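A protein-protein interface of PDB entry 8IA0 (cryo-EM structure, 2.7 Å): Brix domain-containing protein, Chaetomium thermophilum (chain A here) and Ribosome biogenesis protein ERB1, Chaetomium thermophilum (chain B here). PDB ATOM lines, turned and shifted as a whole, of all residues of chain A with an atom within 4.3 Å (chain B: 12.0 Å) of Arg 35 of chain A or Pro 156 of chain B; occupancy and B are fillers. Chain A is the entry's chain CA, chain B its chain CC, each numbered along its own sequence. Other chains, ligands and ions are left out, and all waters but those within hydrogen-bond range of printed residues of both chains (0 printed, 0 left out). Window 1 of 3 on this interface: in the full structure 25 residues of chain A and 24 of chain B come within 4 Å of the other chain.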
ATOM      1  N   LYS A  33     -23.122  31.425  -1.403  1.00  0.00           N
ATOM      2  CA  LYS A  33     -23.637  30.077  -1.606  1.00  0.00           C
ATOM      3  C   LYS A  33     -23.750  29.797  -3.099  1.00  0.00           C
ATOM      4  O   LYS A  33     -24.656  30.304  -3.767  1.00  0.00           O
ATOM      5  CB  LYS A  33     -24.984  29.918  -0.908  1.00  0.00           C
ATOM      6  CG  LYS A  33     -24.912  30.069   0.602  1.00  0.00           C
ATOM      7  CD  LYS A  33     -26.210  29.648   1.268  1.00  0.00           C
ATOM      8  CE  LYS A  33     -27.294  30.689   1.069  1.00  0.00           C
ATOM      9  NZ  LYS A  33     -28.536  30.335   1.806  1.00  0.00           N
ATOM     10  N   GLN A  34     -22.831  28.990  -3.627  1.00  0.00           N
ATOM     11  CA  GLN A  34     -22.811  28.640  -5.042  1.00  0.00           C
ATOM     12  C   GLN A  34     -22.741  27.128  -5.180  1.00  0.00           C
ATOM     13  O   GLN A  34     -21.818  26.497  -4.657  1.00  0.00           O
ATOM     14  CB  GLN A  34     -21.627  29.297  -5.759  1.00  0.00           C
ATOM     15  CG  GLN A  34     -21.640  30.817  -5.742  1.00  0.00           C
ATOM     16  CD  GLN A  34     -22.784  31.408  -6.542  1.00  0.00           C
ATOM     17  OE1 GLN A  34     -23.414  30.724  -7.347  1.00  0.00           O
ATOM     18  NE2 GLN A  34     -23.059  32.686  -6.322  1.00  0.00           N
ATOM     19  N   ARG A  35     -23.709  26.555  -5.889  1.00  0.00           N
ATOM     20  CA  ARG A  35     -23.732  25.132  -6.200  1.00  0.00           C
ATOM     21  C   ARG A  35     -23.812  24.976  -7.711  1.00  0.00           C
ATOM     22  O   ARG A  35     -24.617  25.648  -8.363  1.00  0.00           O
ATOM     23  CB  ARG A  35     -24.911  24.431  -5.520  1.00  0.00           C
ATOM     24  CG  ARG A  35     -24.620  23.951  -4.109  1.00  0.00           C
ATOM     25  CD  ARG A  35     -25.575  22.846  -3.687  1.00  0.00           C
ATOM     26  NE  ARG A  35     -25.199  21.559  -4.253  1.00  0.00           N
ATOM     27  CZ  ARG A  35     -25.739  20.400  -3.906  1.00  0.00           C
ATOM     28  NH1 ARG A  35     -26.691  20.328  -2.992  1.00  0.00           N
ATOM     29  NH2 ARG A  35     -25.315  19.285  -4.493  1.00  0.00           N
ATOM     30  N   VAL A  36     -22.984  24.094  -8.262  1.00  0.00           N
ATOM     31  CA  VAL A  36     -22.832  23.940  -9.702  1.00  0.00           C
ATOM     32  C   VAL A  36     -23.276  22.539 -10.100  1.00  0.00           C
ATOM     33  O   VAL A  36     -23.013  21.568  -9.383  1.00  0.00           O
ATOM     34  CB  VAL A  36     -21.377  24.207 -10.141  1.00  0.00           C
ATOM     35  CG1 VAL A  36     -21.189  23.904 -11.614  1.00  0.00           C
ATOM     36  CG2 VAL A  36     -20.994  25.643  -9.843  1.00  0.00           C
ATOM     37  N   HIS A  61     -17.862  22.375  -5.110  1.00  0.00           N
ATOM     38  CA  HIS A  61     -19.264  22.706  -4.920  1.00  0.00           C
ATOM     39  C   HIS A  61     -20.137  22.209  -6.060  1.00  0.00           C
ATOM     40  O   HIS A  61     -21.341  22.481  -6.068  1.00  0.00           O
ATOM     41  CB  HIS A  61     -19.430  24.218  -4.753  1.00  0.00           C
ATOM     42  CG  HIS A  61     -18.898  25.020  -5.900  1.00  0.00           C
ATOM     43  ND1 HIS A  61     -17.589  24.947  -6.323  1.00  0.00           N
ATOM     44  CD2 HIS A  61     -19.500  25.928  -6.704  1.00  0.00           C
ATOM     45  CE1 HIS A  61     -17.410  25.765  -7.344  1.00  0.00           C
ATOM     46  NE2 HIS A  61     -18.554  26.375  -7.593  1.00  0.00           N
ATOM     47  N   ARG A  63     -21.417  18.950  -8.793  1.00  0.00           N
ATOM     48  CA  ARG A  63     -21.642  17.517  -8.876  1.00  0.00           C
ATOM     49  C   ARG A  63     -21.837  17.101 -10.325  1.00  0.00           C
ATOM     50  O   ARG A  63     -22.341  17.871 -11.148  1.00  0.00           O
ATOM     51  CB  ARG A  63     -22.852  17.084  -8.057  1.00  0.00           C
ATOM     52  CG  ARG A  63     -24.081  17.937  -8.253  1.00  0.00           C
ATOM     53  CD  ARG A  63     -25.231  17.331  -7.487  1.00  0.00           C
ATOM     54  NE  ARG A  63     -25.481  15.969  -7.938  1.00  0.00           N
ATOM     55  CZ  ARG A  63     -25.745  14.950  -7.133  1.00  0.00           C
ATOM     56  NH1 ARG A  63     -25.809  15.105  -5.822  1.00  0.00           N
ATOM     57  NH2 ARG A  63     -25.950  13.745  -7.658  1.00  0.00           N
ATOM     58  N   TYR A  84     -31.517  19.396  -7.712  1.00  0.00           N
ATOM     59  CA  TYR A  84     -30.311  19.164  -6.929  1.00  0.00           C
ATOM     60  C   TYR A  84     -29.826  20.410  -6.198  1.00  0.00           C
ATOM     61  O   TYR A  84     -28.704  20.408  -5.682  1.00  0.00           O
ATOM     62  CB  TYR A  84     -29.198  18.628  -7.830  1.00  0.00           C
ATOM     63  CG  TYR A  84     -29.244  17.133  -8.027  1.00  0.00           C
ATOM     64  CD1 TYR A  84     -28.937  16.266  -6.992  1.00  0.00           C
ATOM     65  CD2 TYR A  84     -29.597  16.589  -9.251  1.00  0.00           C
ATOM     66  CE1 TYR A  84     -28.985  14.898  -7.170  1.00  0.00           C
ATOM     67  CE2 TYR A  84     -29.642  15.225  -9.440  1.00  0.00           C
ATOM     68  CZ  TYR A  84     -29.335  14.384  -8.397  1.00  0.00           C
ATOM     69  OH  TYR A  84     -29.382  13.022  -8.581  1.00  0.00           O
ATOM     70  N   ASN A  85     -30.633  21.473  -6.164  1.00  0.00           N
ATOM     71  CA  ASN A  85     -30.306  22.704  -5.440  1.00  0.00           C
ATOM     72  C   ASN A  85     -29.061  23.379  -6.011  1.00  0.00           C
ATOM     73  O   ASN A  85     -28.211  23.879  -5.273  1.00  0.00           O
ATOM     74  CB  ASN A  85     -30.141  22.438  -3.942  1.00  0.00           C
ATOM     75  CG  ASN A  85     -31.431  22.612  -3.175  1.00  0.00           C
ATOM     76  OD1 ASN A  85     -32.404  23.158  -3.690  1.00  0.00           O
ATOM     77  ND2 ASN A  85     -31.448  22.146  -1.933  1.00  0.00           N
ATOM     78  N   CYS A  86     -28.953  23.397  -7.335  1.00  0.00           N
ATOM     79  CA  CYS A  86     -27.816  23.984  -8.030  1.00  0.00           C
ATOM     80  C   CYS A  86     -28.274  25.212  -8.800  1.00  0.00           C
ATOM     81  O   CYS A  86     -29.259  25.149  -9.542  1.00  0.00           O
ATOM     82  CB  CYS A  86     -27.170  22.975  -8.984  1.00  0.00           C
ATOM     83  SG  CYS A  86     -26.279  21.633  -8.175  1.00  0.00           S
ATOM     84  N   ASN A  87     -27.564  26.323  -8.619  1.00  0.00           N
ATOM     85  CA  ASN A  87     -27.891  27.573  -9.289  1.00  0.00           C
ATOM     86  C   ASN A  87     -26.897  27.933 -10.386  1.00  0.00           C
ATOM     87  O   ASN A  87     -26.937  29.052 -10.903  1.00  0.00           O
ATOM     88  CB  ASN A  87     -27.996  28.706  -8.267  1.00  0.00           C
ATOM     89  CG  ASN A  87     -26.675  29.022  -7.605  1.00  0.00           C
ATOM     90  OD1 ASN A  87     -25.798  28.167  -7.503  1.00  0.00           O
ATOM     91  ND2 ASN A  87     -26.527  30.257  -7.150  1.00  0.00           N
ATOM     92  N   ASN A  88     -26.009  27.012 -10.751  1.00  0.00           N
ATOM     93  CA  ASN A  88     -25.119  27.170 -11.892  1.00  0.00           C
ATOM     94  C   ASN A  88     -25.061  25.856 -12.653  1.00  0.00           C
ATOM     95  O   ASN A  88     -24.888  24.792 -12.052  1.00  0.00           O
ATOM     96  CB  ASN A  88     -23.709  27.585 -11.459  1.00  0.00           C
ATOM     97  CG  ASN A  88     -23.692  28.891 -10.700  1.00  0.00           C
ATOM     98  OD1 ASN A  88     -23.469  29.951 -11.277  1.00  0.00           O
ATOM     99  ND2 ASN A  88     -23.928  28.822  -9.396  1.00  0.00           N
ATOM    100  N   ASP B 152     -38.839  32.098  -8.922  1.00  0.00           N
ATOM    101  CA  ASP B 152     -38.176  32.163  -7.629  1.00  0.00           C
ATOM    102  C   ASP B 152     -36.796  31.519  -7.704  1.00  0.00           C
ATOM    103  O   ASP B 152     -36.584  30.527  -8.406  1.00  0.00           O
ATOM    104  CB  ASP B 152     -39.024  31.486  -6.553  1.00  0.00           C
ATOM    105  CG  ASP B 152     -39.722  30.240  -7.055  1.00  0.00           C
ATOM    106  OD1 ASP B 152     -39.066  29.415  -7.723  1.00  0.00           O
ATOM    107  OD2 ASP B 152     -40.927  30.080  -6.772  1.00  0.00           O
ATOM    108  N   GLU B 153     -35.853  32.101  -6.974  1.00  0.00           N
ATOM    109  CA  GLU B 153     -34.472  31.661  -7.042  1.00  0.00           C
ATOM    110  C   GLU B 153     -34.267  30.370  -6.258  1.00  0.00           C
ATOM    111  O   GLU B 153     -35.110  29.949  -5.462  1.00  0.00           O
ATOM    112  CB  GLU B 153     -33.537  32.747  -6.512  1.00  0.00           C
ATOM    113  CG  GLU B 153     -33.814  34.124  -7.076  1.00  0.00           C
ATOM    114  CD  GLU B 153     -33.123  34.358  -8.402  1.00  0.00           C
ATOM    115  OE1 GLU B 153     -32.138  33.648  -8.692  1.00  0.00           O
ATOM    116  OE2 GLU B 153     -33.563  35.251  -9.155  1.00  0.00           O
ATOM    117  N   ILE B 154     -33.129  29.746  -6.496  1.00  0.00           N
ATOM    118  CA  ILE B 154     -32.738  28.515  -5.820  1.00  0.00           C
ATOM    119  C   ILE B 154     -31.921  28.867  -4.586  1.00  0.00           C
ATOM    120  O   ILE B 154     -31.120  29.806  -4.590  1.00  0.00           O
ATOM    121  CB  ILE B 154     -31.949  27.597  -6.776  1.00  0.00           C
ATOM    122  CG1 ILE B 154     -32.732  27.374  -8.068  1.00  0.00           C
ATOM    123  CG2 ILE B 154     -31.630  26.268  -6.107  1.00  0.00           C
ATOM    124  CD1 ILE B 154     -32.286  26.164  -8.849  1.00  0.00           C
ATOM    125  N   ASP B 155     -32.123  28.103  -3.513  1.00  0.00           N
ATOM    126  CA  ASP B 155     -31.311  28.246  -2.316  1.00  0.00           C
ATOM    127  C   ASP B 155     -30.260  27.149  -2.313  1.00  0.00           C
ATOM    128  O   ASP B 155     -30.598  25.984  -2.057  1.00  0.00           O
ATOM    129  CB  ASP B 155     -32.178  28.158  -1.062  1.00  0.00           C
ATOM    130  CG  ASP B 155     -31.515  28.779   0.150  1.00  0.00           C
ATOM    131  OD1 ASP B 155     -30.339  29.185   0.045  1.00  0.00           O
ATOM    132  OD2 ASP B 155     -32.171  28.861   1.209  1.00  0.00           O
ATOM    133  N   PRO B 156     -28.996  27.455  -2.586  1.00  0.00           N
ATOM    134  CA  PRO B 156     -27.986  26.395  -2.684  1.00  0.00           C
ATOM    135  C   PRO B 156     -27.624  25.809  -1.332  1.00  0.00           C
ATOM    136  O   PRO B 156     -26.588  26.145  -0.751  1.00  0.00           O
ATOM    137  CB  PRO B 156     -26.791  27.107  -3.332  1.00  0.00           C
ATOM    138  CG  PRO B 156     -27.353  28.369  -3.910  1.00  0.00           C
ATOM    139  CD  PRO B 156     -28.449  28.759  -2.983  1.00  0.00           C
ATOM    140  N   VAL B 157     -28.480  24.925  -0.828  1.00  0.00           N
ATOM    141  CA  VAL B 157     -28.257  24.233   0.431  1.00  0.00           C
ATOM    142  C   VAL B 157     -28.357  22.737   0.177  1.00  0.00           C
ATOM    143  O   VAL B 157     -28.981  22.285  -0.784  1.00  0.00           O
ATOM    144  CB  VAL B 157     -29.256  24.664   1.523  1.00  0.00           C
ATOM    145  CG1 VAL B 157     -28.922  26.058   2.024  1.00  0.00           C
ATOM    146  CG2 VAL B 157     -30.678  24.607   0.990  1.00  0.00           C
ATOM    147  N   TYR B 158     -27.728  21.968   1.058  1.00  0.00           N
ATOM    148  CA  TYR B 158     -27.687  20.515   0.929  1.00  0.00           C
ATOM    149  C   TYR B 158     -28.849  19.930   1.719  1.00  0.00           C
ATOM    150  O   TYR B 158     -28.934  20.096   2.938  1.00  0.00           O
ATOM    151  CB  TYR B 158     -26.348  19.971   1.415  1.00  0.00           C
ATOM    152  CG  TYR B 158     -25.180  20.339   0.531  1.00  0.00           C
ATOM    153  CD1 TYR B 158     -24.640  21.616   0.557  1.00  0.00           C
ATOM    154  CD2 TYR B 158     -24.616  19.410  -0.328  1.00  0.00           C
ATOM    155  CE1 TYR B 158     -23.577  21.957  -0.249  1.00  0.00           C
ATOM    156  CE2 TYR B 158     -23.553  19.742  -1.138  1.00  0.00           C
ATOM    157  CZ  TYR B 158     -23.037  21.017  -1.094  1.00  0.00           C
ATOM    158  OH  TYR B 158     -21.975  21.353  -1.898  1.00  0.00           O
ATOM    159  N   ASP B 159     -29.750  19.244   1.024  1.00  0.00           N
ATOM    160  CA  ASP B 159     -30.867  18.575   1.676  1.00  0.00           C
ATOM    161  C   ASP B 159     -30.365  17.384   2.483  1.00  0.00           C
ATOM    162  O   ASP B 159     -29.244  16.921   2.286  1.00  0.00           O
ATOM    163  CB  ASP B 159     -31.905  18.128   0.648  1.00  0.00           C
ATOM    164  CG  ASP B 159     -32.694  19.287   0.077  1.00  0.00           C
ATOM    165  OD1 ASP B 159     -32.839  20.310   0.777  1.00  0.00           O
ATOM    166  OD2 ASP B 159     -33.171  19.175  -1.070  1.00  0.00           O
ATOM    167  N   SEP B 160     -31.205  16.883   3.383  1.00  0.00           N
ATOM    168  CA  SEP B 160     -30.806  15.840   4.322  1.00  0.00           C
ATOM    169  CB  SEP B 160     -31.826  15.743   5.455  1.00  0.00           C
ATOM    170  OG  SEP B 160     -32.996  15.075   5.017  1.00  0.00           O
ATOM    171  C   SEP B 160     -30.648  14.465   3.681  1.00  0.00           C
ATOM    172  O   SEP B 160     -30.755  13.449   4.363  1.00  0.00           O
ATOM    173  P   SEP B 160     -34.305  15.914   5.425  1.00  0.00           P
ATOM    174  O1P SEP B 160     -35.612  15.164   4.863  1.00  0.00           O
ATOM    175  O2P SEP B 160     -34.218  17.388   4.785  1.00  0.00           O
ATOM    176  O3P SEP B 160     -34.396  16.026   7.028  1.00  0.00           O
ATOM    177  N   ASP B 161     -30.393  14.428   2.379  1.00  0.00           N
ATOM    178  CA  ASP B 161     -30.304  13.161   1.669  1.00  0.00           C
ATOM    179  C   ASP B 161     -29.276  13.210   0.547  1.00  0.00           C
ATOM    180  O   ASP B 161     -29.199  12.297  -0.274  1.00  0.00           O
ATOM    181  CB  ASP B 161     -31.671  12.770   1.106  1.00  0.00           C
ATOM    182  CG  ASP B 161     -32.163  13.734   0.049  1.00  0.00           C
ATOM    183  OD1 ASP B 161     -32.253  14.943   0.341  1.00  0.00           O
ATOM    184  OD2 ASP B 161     -32.459  13.285  -1.077  1.00  0.00           O
ATOM    185  N   ASP B 162     -28.485  14.275   0.515  1.00  0.00           N
ATOM    186  CA  ASP B 162     -27.423  14.398  -0.473  1.00  0.00           C
ATOM    187  C   ASP B 162     -26.232  13.538  -0.072  1.00  0.00           C
ATOM    188  O   ASP B 162     -26.150  13.072   1.064  1.00  0.00           O
ATOM    189  CB  ASP B 162     -26.996  15.857  -0.629  1.00  0.00           C
ATOM    190  CG  ASP B 162     -27.585  16.506  -1.862  1.00  0.00           C
ATOM    191  OD1 ASP B 162     -28.750  16.203  -2.197  1.00  0.00           O
ATOM    192  OD2 ASP B 162     -26.883  17.318  -2.501  1.00  0.00           O
ATOM    193  N   TPO B 163     -25.312  13.324  -1.007  1.00  0.00           N
ATOM    194  CA  TPO B 163     -24.103  12.568  -0.720  1.00  0.00           C
ATOM    195  CB  TPO B 163     -23.453  12.065  -2.017  1.00  0.00           C
ATOM    196  CG2 TPO B 163     -23.354  10.534  -2.022  1.00  0.00           C
ATOM    197  OG1 TPO B 163     -24.094  12.618  -3.184  1.00  0.00           O
ATOM    198  P   TPO B 163     -25.309  11.746  -3.798  1.00  0.00           P
ATOM    199  O1P TPO B 163     -26.250  11.117  -2.652  1.00  0.00           O
ATOM    200  O2P TPO B 163     -26.150  12.654  -4.606  1.00  0.00           O
ATOM    201  O3P TPO B 163     -24.753  10.594  -4.775  1.00  0.00           O
ATOM    202  C   TPO B 163     -23.115  13.421   0.070  1.00  0.00           C
ATOM    203  O   TPO B 163     -22.270  12.900   0.793  1.00  0.00           O
ATOM    204  N   ASP B 164     -23.233  14.737  -0.076  1.00  0.00           N
ATOM    205  CA  ASP B 164     -22.301  15.667   0.551  1.00  0.00           C
ATOM    206  C   ASP B 164     -22.960  16.445   1.682  1.00  0.00           C
ATOM    207  O   ASP B 164     -22.487  17.512   2.071  1.00  0.00           O
ATOM    208  CB  ASP B 164     -21.738  16.636  -0.490  1.00  0.00           C
ATOM    209  CG  ASP B 164     -21.037  15.924  -1.627  1.00  0.00           C
ATOM    210  OD1 ASP B 164     -20.370  14.901  -1.369  1.00  0.00           O
ATOM    211  OD2 ASP B 164     -21.152  16.389  -2.781  1.00  0.00           O
ATOM    212  N   TYR B 165     -24.065  15.909   2.200  1.00  0.00           N
ATOM    213  CA  TYR B 165     -24.760  16.564   3.303  1.00  0.00           C
ATOM    214  C   TYR B 165     -23.901  16.595   4.560  1.00  0.00           C
ATOM    215  O   TYR B 165     -23.826  17.620   5.245  1.00  0.00           O
ATOM    216  CB  TYR B 165     -26.088  15.856   3.568  1.00  0.00           C
ATOM    217  CG  TYR B 165     -26.832  16.345   4.784  1.00  0.00           C
ATOM    218  CD1 TYR B 165     -27.452  17.584   4.791  1.00  0.00           C
ATOM    219  CD2 TYR B 165     -26.932  15.558   5.918  1.00  0.00           C
ATOM    220  CE1 TYR B 165     -28.137  18.030   5.900  1.00  0.00           C
ATOM    221  CE2 TYR B 165     -27.616  15.994   7.030  1.00  0.00           C
ATOM    222  CZ  TYR B 165     -28.219  17.229   7.015  1.00  0.00           C
ATOM    223  OH  TYR B 165     -28.902  17.670   8.124  1.00  0.00           O
ATOM    224  N   ASN B 166     -23.245  15.483   4.878  1.00  0.00           N
ATOM    225  CA  ASN B 166     -22.322  15.398   6.005  1.00  0.00           C
ATOM    226  C   ASN B 166     -20.919  15.199   5.448  1.00  0.00           C
ATOM    227  O   ASN B 166     -20.589  14.117   4.952  1.00  0.00           O
ATOM    228  CB  ASN B 166     -22.702  14.261   6.950  1.00  0.00           C
ATOM    229  CG  ASN B 166     -23.918  14.584   7.789  1.00  0.00           C
ATOM    230  OD1 ASN B 166     -23.932  15.565   8.530  1.00  0.00           O
ATOM    231  ND2 ASN B 166     -24.946  13.750   7.685  1.00  0.00           N
ATOM    232  N   VAL B 167     -20.096  16.240   5.531  1.00  0.00           N
ATOM    233  CA  VAL B 167     -18.734  16.183   5.009  1.00  0.00           C
ATOM    234  C   VAL B 167     -17.754  16.083   6.173  1.00  0.00           C
ATOM    235  O   VAL B 167     -17.974  16.704   7.223  1.00  0.00           O
ATOM    236  CB  VAL B 167     -18.429  17.396   4.119  1.00  0.00           C
ATOM    237  CG1 VAL B 167     -19.042  17.195   2.746  1.00  0.00           C
ATOM    238  CG2 VAL B 167     -18.973  18.654   4.750  1.00  0.00           C
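No residue of chain B comes within 4 Å of Gln 34 of chain A.
Of chain B, only Pro 156, Val 157, Tyr 158 and Asp 162 come within 4 Å of Arg 35 of chain A.
Of chain B, only TPO 163 comes within 4 Å of Arg 63 of chain A.
Asn 85 of chain A touches just these residues of chain B: Ile 154, Asp 155, Pro 156, Val 157 and Asp 159.
Cys 86 of chain A touches just one residue of chain B: Ile 154 (3.3 Å).
Of chain A, only Lys 33, Arg 35, Asn 85 and Asn 87 come within 4 Å of Pro 156 of chain B.
Of the printed residues of chain A, Val 157 of chain B touches Arg 35 and Asn 85.
Printed residues of chain A within 4 Å of Tyr 158 of chain B: Arg 35.
Of the printed residues of chain A, TPO 163 of chain B touches Arg 63.
The nearest printed residue of chain A that does not touch Pro 156 of chain B is Gln 34 of chain A (4.4 Å).
The nearest printed residue of chain A that does not touch TPO 163 of chain B is Tyr 84 of chain A (4.4 Å).
Of the 16 printed residues of chain B, 8 touch a printed residue of chain A.
Among the printed residues, pairs that only touch across the chains: Cys 86 of chain A with Ile 154 of chain B (3.3 Å), Lys 33 of chain A with Pro 156 of chain B (3.3 Å), Arg 35 of chain A with Tyr 158 of chain B (3.5 Å), Asn 85 of chain A with Asp 159 of chain B (3.5 Å), Asn 85 of chain A with Pro 156 of chain B (3.6 Å), Asn 85 of chain A with Asp 155 of chain B (3.6 Å), Arg 35 of chain A with Val 157 of chain B (3.7 Å), Asn 87 of chain A with Pro 156 of chain B (3.8 Å), Asn 85 of chain A with Ile 154 of chain B (3.9 Å) and Arg 35 of chain A with Pro 156 of chain B (3.9 Å).
N of Arg 63 of chain A is in hydrogen-bond range of O of Val 36 of chain A.
The side-chain amide nitrogen (ND2) of Asn 87 of chain A lies within hydrogen-bond range of the side-chain amide oxygen (OE1) of Gln 34 of chain A.
The backbone carbonyl oxygen of Arg 35 of chain A sits close to the side-chain amide oxygen of Asn 87 of chain A, at 2.9 Å.
OD1 of Asn 87 of chain A lies within hydrogen-bond range of ND2 of Asn 88 of chain A (2.7 Å).
O of Val 36 of chain A is in hydrogen-bond range of SG of Cys 86 of chain A (3.5 Å).
The backbone carbonyl oxygen (O) of Arg 35 of chain A lies within hydrogen-bond range of the backbone NH (N) of Asn 88 of chain A (3.1 Å).
NH1 of Arg 63 of chain A lies close to O2P of TPO 163 of chain B, at 2.8 Å.
The side-chain carboxylate (OD2) of Asp 162 of chain B is in salt-bridge range of the guanidinium group (NH1) of Arg 35 of chain A.
The side-chain amide nitrogen (ND2) of Asn 85 of chain A sits at hydrogen-bond distance from the backbone carbonyl oxygen (O) of Val 157 of chain B (2.7 Å).
The side-chain carboxylate (OD1) of Asp 155 of chain B lies within salt-bridge range of the side-chain amino group (NZ) of Lys 33 of chain A (2.8 Å).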
